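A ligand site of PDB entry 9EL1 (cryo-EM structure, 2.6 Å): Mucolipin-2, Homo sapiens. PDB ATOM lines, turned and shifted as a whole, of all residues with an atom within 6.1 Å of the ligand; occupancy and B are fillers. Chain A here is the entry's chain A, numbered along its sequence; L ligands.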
ATOM      1  N   PHE A  47      -6.296  16.538 -32.195  1.00  0.00           N
ATOM      2  CA  PHE A  47      -7.344  15.664 -31.691  1.00  0.00           C
ATOM      3  C   PHE A  47      -8.461  16.466 -31.038  1.00  0.00           C
ATOM      4  O   PHE A  47      -9.639  16.088 -31.136  1.00  0.00           O
ATOM      5  CB  PHE A  47      -6.766  14.664 -30.689  1.00  0.00           C
ATOM      6  CG  PHE A  47      -7.729  13.576 -30.302  1.00  0.00           C
ATOM      7  CD1 PHE A  47      -8.439  12.887 -31.261  1.00  0.00           C
ATOM      8  CD2 PHE A  47      -7.930  13.259 -28.965  1.00  0.00           C
ATOM      9  CE1 PHE A  47      -9.329  11.891 -30.904  1.00  0.00           C
ATOM     10  CE2 PHE A  47      -8.814  12.265 -28.596  1.00  0.00           C
ATOM     11  CZ  PHE A  47      -9.520  11.583 -29.566  1.00  0.00           C
ATOM     12  N   TYR A  48      -8.128  17.557 -30.363  1.00  0.00           N
ATOM     13  CA  TYR A  48      -9.118  18.275 -29.571  1.00  0.00           C
ATOM     14  C   TYR A  48     -10.203  18.926 -30.421  1.00  0.00           C
ATOM     15  O   TYR A  48     -11.337  19.065 -29.945  1.00  0.00           O
ATOM     16  CB  TYR A  48      -8.428  19.352 -28.721  1.00  0.00           C
ATOM     17  CG  TYR A  48      -9.375  20.168 -27.886  1.00  0.00           C
ATOM     18  CD1 TYR A  48      -9.915  19.661 -26.709  1.00  0.00           C
ATOM     19  CD2 TYR A  48      -9.740  21.446 -28.269  1.00  0.00           C
ATOM     20  CE1 TYR A  48     -10.782  20.402 -25.939  1.00  0.00           C
ATOM     21  CE2 TYR A  48     -10.617  22.199 -27.511  1.00  0.00           C
ATOM     22  CZ  TYR A  48     -11.134  21.667 -26.342  1.00  0.00           C
ATOM     23  OH  TYR A  48     -11.997  22.416 -25.583  1.00  0.00           O
ATOM     24  N   PRO A  52     -16.478  14.466 -33.594  1.00  0.00           N
ATOM     25  CA  PRO A  52     -16.488  13.176 -32.894  1.00  0.00           C
ATOM     26  C   PRO A  52     -16.405  11.992 -33.844  1.00  0.00           C
ATOM     27  O   PRO A  52     -15.893  10.935 -33.487  1.00  0.00           O
ATOM     28  CB  PRO A  52     -17.832  13.197 -32.147  1.00  0.00           C
ATOM     29  CG  PRO A  52     -18.668  14.197 -32.887  1.00  0.00           C
ATOM     30  CD  PRO A  52     -17.703  15.246 -33.342  1.00  0.00           C
ATOM     31  N   LYS A  55     -12.790  11.856 -34.467  1.00  0.00           N
ATOM     32  CA  LYS A  55     -12.111  11.376 -33.279  1.00  0.00           C
ATOM     33  C   LYS A  55     -12.141   9.859 -33.213  1.00  0.00           C
ATOM     34  O   LYS A  55     -11.369   9.243 -32.476  1.00  0.00           O
ATOM     35  CB  LYS A  55     -12.719  11.980 -32.009  1.00  0.00           C
ATOM     36  CG  LYS A  55     -12.510  13.478 -31.868  1.00  0.00           C
ATOM     37  CD  LYS A  55     -12.743  13.918 -30.433  1.00  0.00           C
ATOM     38  CE  LYS A  55     -12.817  15.431 -30.337  1.00  0.00           C
ATOM     39  NZ  LYS A  55     -12.542  15.909 -28.956  1.00  0.00           N
ATOM     40  N   ARG A  59      -8.008   8.223 -33.185  1.00  0.00           N
ATOM     41  CA  ARG A  59      -7.599   7.332 -32.101  1.00  0.00           C
ATOM     42  C   ARG A  59      -8.520   6.131 -31.938  1.00  0.00           C
ATOM     43  O   ARG A  59      -8.277   5.298 -31.050  1.00  0.00           O
ATOM     44  CB  ARG A  59      -7.523   8.107 -30.782  1.00  0.00           C
ATOM     45  CG  ARG A  59      -6.157   8.726 -30.508  1.00  0.00           C
ATOM     46  CD  ARG A  59      -6.271  10.134 -29.959  1.00  0.00           C
ATOM     47  NE  ARG A  59      -4.992  10.653 -29.499  1.00  0.00           N
ATOM     48  CZ  ARG A  59      -4.323  11.644 -30.085  1.00  0.00           C
ATOM     49  NH1 ARG A  59      -4.765  12.209 -31.196  1.00  0.00           N
ATOM     50  NH2 ARG A  59      -3.181  12.054 -29.550  1.00  0.00           N
ATOM     51  N   GLN A  61     -11.841   5.427 -30.851  1.00  0.00           N
ATOM     52  CA  GLN A  61     -12.440   5.234 -29.547  1.00  0.00           C
ATOM     53  C   GLN A  61     -13.940   5.487 -29.622  1.00  0.00           C
ATOM     54  O   GLN A  61     -14.419   6.233 -30.482  1.00  0.00           O
ATOM     55  CB  GLN A  61     -11.798   6.140 -28.481  1.00  0.00           C
ATOM     56  CG  GLN A  61     -12.428   7.524 -28.380  1.00  0.00           C
ATOM     57  CD  GLN A  61     -12.076   8.405 -29.556  1.00  0.00           C
ATOM     58  OE1 GLN A  61     -10.916   8.726 -29.772  1.00  0.00           O
ATOM     59  NE2 GLN A  61     -13.083   8.787 -30.324  1.00  0.00           N
ATOM     60  N   ILE A  62     -14.678   4.847 -28.731  1.00  0.00           N
ATOM     61  CA  ILE A  62     -16.151   4.936 -28.745  1.00  0.00           C
ATOM     62  C   ILE A  62     -16.577   6.309 -28.265  1.00  0.00           C
ATOM     63  O   ILE A  62     -16.034   6.809 -27.267  1.00  0.00           O
ATOM     64  CB  ILE A  62     -16.754   3.822 -27.874  1.00  0.00           C
ATOM     65  CG1 ILE A  62     -17.114   2.608 -28.734  1.00  0.00           C
ATOM     66  CG2 ILE A  62     -17.980   4.320 -27.130  1.00  0.00           C
ATOM     67  CD1 ILE A  62     -15.949   1.984 -29.457  1.00  0.00           C
ATOM     68  N   PRO A  63     -17.522   6.967 -28.948  1.00  0.00           N
ATOM     69  CA  PRO A  63     -18.009   8.270 -28.473  1.00  0.00           C
ATOM     70  C   PRO A  63     -19.161   8.146 -27.490  1.00  0.00           C
ATOM     71  O   PRO A  63     -20.325   8.295 -27.884  1.00  0.00           O
ATOM     72  CB  PRO A  63     -18.438   8.958 -29.773  1.00  0.00           C
ATOM     73  CG  PRO A  63     -18.800   7.817 -30.717  1.00  0.00           C
ATOM     74  CD  PRO A  63     -18.233   6.530 -30.166  1.00  0.00           C
ATOM     75  N   TRP A  64     -18.852   7.867 -26.224  1.00  0.00           N
ATOM     76  CA  TRP A  64     -19.894   7.700 -25.221  1.00  0.00           C
ATOM     77  C   TRP A  64     -20.709   8.966 -25.050  1.00  0.00           C
ATOM     78  O   TRP A  64     -21.934   8.913 -24.851  1.00  0.00           O
ATOM     79  CB  TRP A  64     -19.279   7.282 -23.886  1.00  0.00           C
ATOM     80  CG  TRP A  64     -18.960   5.826 -23.800  1.00  0.00           C
ATOM     81  CD1 TRP A  64     -19.843   4.790 -23.789  1.00  0.00           C
ATOM     82  CD2 TRP A  64     -17.656   5.233 -23.694  1.00  0.00           C
ATOM     83  NE1 TRP A  64     -19.171   3.598 -23.700  1.00  0.00           N
ATOM     84  CE2 TRP A  64     -17.829   3.847 -23.637  1.00  0.00           C
ATOM     85  CE3 TRP A  64     -16.360   5.761 -23.652  1.00  0.00           C
ATOM     86  CZ2 TRP A  64     -16.759   2.963 -23.537  1.00  0.00           C
ATOM     87  CZ3 TRP A  64     -15.292   4.891 -23.552  1.00  0.00           C
ATOM     88  CH2 TRP A  64     -15.498   3.499 -23.492  1.00  0.00           C
ATOM     89  N   LYS A  65     -20.056  10.120 -25.125  1.00  0.00           N
ATOM     90  CA  LYS A  65     -20.714  11.405 -24.896  1.00  0.00           C
ATOM     91  C   LYS A  65     -21.652  11.786 -26.034  1.00  0.00           C
ATOM     92  O   LYS A  65     -22.157  12.912 -26.072  1.00  0.00           O
ATOM     93  CB  LYS A  65     -19.671  12.506 -24.687  1.00  0.00           C
ATOM     94  CG  LYS A  65     -20.080  13.538 -23.659  1.00  0.00           C
ATOM     95  CD  LYS A  65     -18.960  14.526 -23.408  1.00  0.00           C
ATOM     96  CE  LYS A  65     -17.632  13.809 -23.295  1.00  0.00           C
ATOM     97  NZ  LYS A  65     -16.620  14.616 -22.568  1.00  0.00           N
ATOM     98  N   LEU A  66     -21.885  10.886 -26.989  1.00  0.00           N
ATOM     99  CA  LEU A  66     -22.865  11.157 -28.029  1.00  0.00           C
ATOM    100  C   LEU A  66     -24.035  10.180 -27.914  1.00  0.00           C
ATOM    101  O   LEU A  66     -25.200  10.587 -27.950  1.00  0.00           O
ATOM    102  CB  LEU A  66     -22.228  11.058 -29.412  1.00  0.00           C
ATOM    103  CG  LEU A  66     -23.073  11.572 -30.573  1.00  0.00           C
ATOM    104  CD1 LEU A  66     -22.326  12.623 -31.373  1.00  0.00           C
ATOM    105  CD2 LEU A  66     -23.499  10.414 -31.471  1.00  0.00           C
ATOM    106  N   LEU A 307     -18.679  12.676 -17.166  1.00  0.00           N
ATOM    107  CA  LEU A 307     -17.941  12.740 -18.427  1.00  0.00           C
ATOM    108  C   LEU A 307     -17.673  14.191 -18.830  1.00  0.00           C
ATOM    109  O   LEU A 307     -16.564  14.534 -19.233  1.00  0.00           O
ATOM    110  CB  LEU A 307     -18.721  12.015 -19.520  1.00  0.00           C
ATOM    111  CG  LEU A 307     -18.845  10.499 -19.372  1.00  0.00           C
ATOM    112  CD1 LEU A 307     -19.304   9.868 -20.670  1.00  0.00           C
ATOM    113  CD2 LEU A 307     -17.531   9.893 -18.904  1.00  0.00           C
ATOM    114  N   ARG A 310     -15.126  15.904 -16.651  1.00  0.00           N
ATOM    115  CA  ARG A 310     -13.798  15.439 -17.041  1.00  0.00           C
ATOM    116  C   ARG A 310     -13.238  16.254 -18.197  1.00  0.00           C
ATOM    117  O   ARG A 310     -12.099  16.714 -18.164  1.00  0.00           O
ATOM    118  CB  ARG A 310     -13.845  13.959 -17.403  1.00  0.00           C
ATOM    119  CG  ARG A 310     -12.491  13.352 -17.727  1.00  0.00           C
ATOM    120  CD  ARG A 310     -12.536  12.549 -19.018  1.00  0.00           C
ATOM    121  NE  ARG A 310     -11.276  11.882 -19.299  1.00  0.00           N
ATOM    122  CZ  ARG A 310     -11.135  10.562 -19.406  1.00  0.00           C
ATOM    123  NH1 ARG A 310     -12.168   9.749 -19.269  1.00  0.00           N
ATOM    124  NH2 ARG A 310      -9.935  10.058 -19.665  1.00  0.00           N
ATOM    125  N   SER A 311     -14.050  16.441 -19.250  1.00  0.00           N
ATOM    126  CA  SER A 311     -13.605  17.174 -20.428  1.00  0.00           C
ATOM    127  C   SER A 311     -13.220  18.603 -20.079  1.00  0.00           C
ATOM    128  O   SER A 311     -12.169  19.100 -20.499  1.00  0.00           O
ATOM    129  CB  SER A 311     -14.705  17.153 -21.495  1.00  0.00           C
ATOM    130  OG  SER A 311     -14.844  15.862 -22.048  1.00  0.00           O
ATOM    131  N   LEU A 314      -9.988  18.509 -18.270  1.00  0.00           N
ATOM    132  CA  LEU A 314      -8.894  18.100 -19.160  1.00  0.00           C
ATOM    133  C   LEU A 314      -8.643  19.141 -20.243  1.00  0.00           C
ATOM    134  O   LEU A 314      -7.497  19.286 -20.699  1.00  0.00           O
ATOM    135  CB  LEU A 314      -9.205  16.742 -19.789  1.00  0.00           C
ATOM    136  CG  LEU A 314      -9.234  15.527 -18.855  1.00  0.00           C
ATOM    137  CD1 LEU A 314      -8.906  14.262 -19.640  1.00  0.00           C
ATOM    138  CD2 LEU A 314      -8.278  15.691 -17.693  1.00  0.00           C
ATOM    139  N   ASN A 344     -15.501  25.187 -23.520  1.00  0.00           N
ATOM    140  CA  ASN A 344     -16.691  24.821 -24.272  1.00  0.00           C
ATOM    141  C   ASN A 344     -17.909  25.194 -23.447  1.00  0.00           C
ATOM    142  O   ASN A 344     -18.157  24.593 -22.396  1.00  0.00           O
ATOM    143  CB  ASN A 344     -16.687  23.337 -24.627  1.00  0.00           C
ATOM    144  CG  ASN A 344     -17.540  23.017 -25.836  1.00  0.00           C
ATOM    145  OD1 ASN A 344     -17.606  21.868 -26.280  1.00  0.00           O
ATOM    146  ND2 ASN A 344     -18.203  24.027 -26.371  1.00  0.00           N
ATOM    147  N   TYR A 347     -20.736  22.370 -23.015  1.00  0.00           N
ATOM    148  CA  TYR A 347     -20.641  21.487 -21.869  1.00  0.00           C
ATOM    149  C   TYR A 347     -21.075  22.169 -20.576  1.00  0.00           C
ATOM    150  O   TYR A 347     -21.598  21.498 -19.682  1.00  0.00           O
ATOM    151  CB  TYR A 347     -19.218  20.948 -21.723  1.00  0.00           C
ATOM    152  CG  TYR A 347     -18.879  19.910 -22.753  1.00  0.00           C
ATOM    153  CD1 TYR A 347     -19.881  19.285 -23.491  1.00  0.00           C
ATOM    154  CD2 TYR A 347     -17.570  19.537 -22.986  1.00  0.00           C
ATOM    155  CE1 TYR A 347     -19.585  18.329 -24.430  1.00  0.00           C
ATOM    156  CE2 TYR A 347     -17.254  18.570 -23.934  1.00  0.00           C
ATOM    157  CZ  TYR A 347     -18.272  17.972 -24.652  1.00  0.00           C
ATOM    158  OH  TYR A 347     -17.976  17.017 -25.591  1.00  0.00           O
ATOM    159  N   ARG A 395     -25.044  21.150 -30.727  1.00  0.00           N
ATOM    160  CA  ARG A 395     -23.592  20.943 -30.682  1.00  0.00           C
ATOM    161  C   ARG A 395     -23.149  19.830 -31.611  1.00  0.00           C
ATOM    162  O   ARG A 395     -22.077  19.902 -32.218  1.00  0.00           O
ATOM    163  CB  ARG A 395     -23.144  20.620 -29.265  1.00  0.00           C
ATOM    164  CG  ARG A 395     -21.675  20.859 -29.042  1.00  0.00           C
ATOM    165  CD  ARG A 395     -21.211  20.229 -27.746  1.00  0.00           C
ATOM    166  NE  ARG A 395     -19.764  20.294 -27.589  1.00  0.00           N
ATOM    167  CZ  ARG A 395     -18.926  19.350 -28.019  1.00  0.00           C
ATOM    168  NH1 ARG A 395     -19.361  18.259 -28.606  1.00  0.00           N
ATOM    169  NH2 ARG A 395     -17.620  19.533 -27.853  1.00  0.00           N
ATOM    170  N   TYR A 396     -23.964  18.784 -31.749  1.00  0.00           N
ATOM    171  CA  TYR A 396     -23.625  17.641 -32.584  1.00  0.00           C
ATOM    172  C   TYR A 396     -24.093  17.837 -34.011  1.00  0.00           C
ATOM    173  O   TYR A 396     -24.230  16.887 -34.790  1.00  0.00           O
ATOM    174  CB  TYR A 396     -24.196  16.375 -31.966  1.00  0.00           C
ATOM    175  CG  TYR A 396     -23.638  16.092 -30.590  1.00  0.00           C
ATOM    176  CD1 TYR A 396     -22.409  16.619 -30.194  1.00  0.00           C
ATOM    177  CD2 TYR A 396     -24.341  15.323 -29.673  1.00  0.00           C
ATOM    178  CE1 TYR A 396     -21.900  16.371 -28.936  1.00  0.00           C
ATOM    179  CE2 TYR A 396     -23.839  15.081 -28.403  1.00  0.00           C
ATOM    180  CZ  TYR A 396     -22.619  15.611 -28.044  1.00  0.00           C
ATOM    181  OH  TYR A 396     -22.106  15.370 -26.797  1.00  0.00           O
ATOM    182  N   TYR A 399     -20.156  21.199 -35.753  1.00  0.00           N
ATOM    183  CA  TYR A 399     -18.949  20.962 -36.537  1.00  0.00           C
ATOM    184  C   TYR A 399     -19.241  20.900 -38.033  1.00  0.00           C
ATOM    185  O   TYR A 399     -18.368  21.219 -38.840  1.00  0.00           O
ATOM    186  CB  TYR A 399     -18.240  19.666 -36.126  1.00  0.00           C
ATOM    187  CG  TYR A 399     -18.064  19.452 -34.645  1.00  0.00           C
ATOM    188  CD1 TYR A 399     -19.000  18.750 -33.896  1.00  0.00           C
ATOM    189  CD2 TYR A 399     -16.915  19.898 -34.006  1.00  0.00           C
ATOM    190  CE1 TYR A 399     -18.817  18.530 -32.548  1.00  0.00           C
ATOM    191  CE2 TYR A 399     -16.721  19.687 -32.657  1.00  0.00           C
ATOM    192  CZ  TYR A 399     -17.672  19.004 -31.928  1.00  0.00           C
ATOM    193  OH  TYR A 399     -17.482  18.799 -30.585  1.00  0.00           O
HETATM  194  C1  LIG L   1     -13.623  12.023 -24.718  1.00  0.00           C
HETATM  195  C2  LIG L   1     -14.093  13.141 -25.659  1.00  0.00           C
HETATM  196  C3  LIG L   1     -13.148  14.349 -25.634  1.00  0.00           C
HETATM  197  C4  LIG L   1     -11.701  13.943 -25.919  1.00  0.00           C
HETATM  198  C5  LIG L   1     -11.221  12.834 -24.977  1.00  0.00           C
HETATM  199  C6  LIG L   1     -12.171  11.618 -24.974  1.00  0.00           C
HETATM  200  O1  LIG L   1     -14.451  10.900 -24.902  1.00  0.00           O
HETATM  201  O2  LIG L   1     -14.148  12.631 -26.968  1.00  0.00           O
HETATM  202  O3  LIG L   1     -13.561  15.267 -26.614  1.00  0.00           O
HETATM  203  O4  LIG L   1     -10.880  15.063 -25.748  1.00  0.00           O
HETATM  204  O5  LIG L   1      -9.951  12.406 -25.399  1.00  0.00           O
HETATM  205  O6  LIG L   1     -11.768  10.730 -23.961  1.00  0.00           O
HETATM  206  P1  LIG L   1     -15.322  10.342 -23.627  1.00  0.00           P
HETATM  207  O7  LIG L   1     -16.635   9.792 -24.136  1.00  0.00           O
HETATM  208  O8  LIG L   1     -15.590  11.456 -22.655  1.00  0.00           O
HETATM  209  O9  LIG L   1     -14.481   9.141 -22.873  1.00  0.00           O
HETATM  210  P2  LIG L   1     -14.914  16.168 -26.328  1.00  0.00           P
HETATM  211  O10 LIG L   1     -16.139  15.407 -26.802  1.00  0.00           O
HETATM  212  O11 LIG L   1     -15.039  16.437 -24.852  1.00  0.00           O
HETATM  213  O12 LIG L   1     -14.825  17.478 -27.067  1.00  0.00           O
HETATM  214  P3  LIG L   1      -8.838  12.008 -24.264  1.00  0.00           P
HETATM  215  O13 LIG L   1      -7.528  11.676 -24.934  1.00  0.00           O
HETATM  216  O14 LIG L   1      -8.643  13.167 -23.322  1.00  0.00           O
HETATM  217  O15 LIG L   1      -9.320  10.797 -23.492  1.00  0.00           O
HETATM  218  C7  LIG L   1     -14.905   8.719 -21.611  1.00  0.00           C
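NH1 of Arg 395 is in hydrogen-bond range of OH of Tyr 399 (2.8 Å).
O of Lys 55 lies within hydrogen-bond range of NE2 of Gln 61, at 2.8 Å.
The backbone carbonyl oxygen (O) of Lys 65 lies within hydrogen-bond range of the side-chain hydroxyl (OH) of Tyr 396 (2.6 Å).
The guanidinium group (NH2) of Arg 395 is in hydrogen-bond range of the side-chain hydroxyl (OH) of Tyr 347 (3.4 Å).
The side-chain amide oxygen (OD1) of Asn 344 sits at hydrogen-bond distance from the guanidinium group (NH2) of Arg 395 (2.8 Å).
O of Leu 307 is in hydrogen-bond range of NZ of Lys 65, at 3.3 Å.
The side-chain hydroxyl (OG) of Ser 311 sits at hydrogen-bond distance from an oxygen (O11) of the ligand (2.9 Å).
An oxygen (O11) of the ligand is in salt-bridge range of the side-chain amino group (NZ) of Lys 65.
OH of Tyr 347 is in hydrogen-bond range of O10 of the ligand (2.7 Å).
The guanidinium group (NH2) of Arg 395 is in salt-bridge range of an oxygen (O12) of the ligand, at 3.6 Å.
The guanidinium group (NH2) of Arg 310 is in salt-bridge range of an oxygen (O15) of the ligand (3.9 Å).
NZ of Lys 55 is in salt-bridge range of O12 of the ligand, 3.4 Å away.
Phe 47 touches the ligand.
Trp 64 touches the ligand (N to O7, 3.6 Å).
Leu 307 touches the ligand.
Leu 314 touches the ligand (CD1 to O14, 3.9 Å).
Hydrophobic or aromatic side chains that line the ligand: Phe 47, Trp 64, Leu 307, Leu 314 and Tyr 347.
Along chain A the residues within 4 Å of the ligand span positions 47 to 395.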
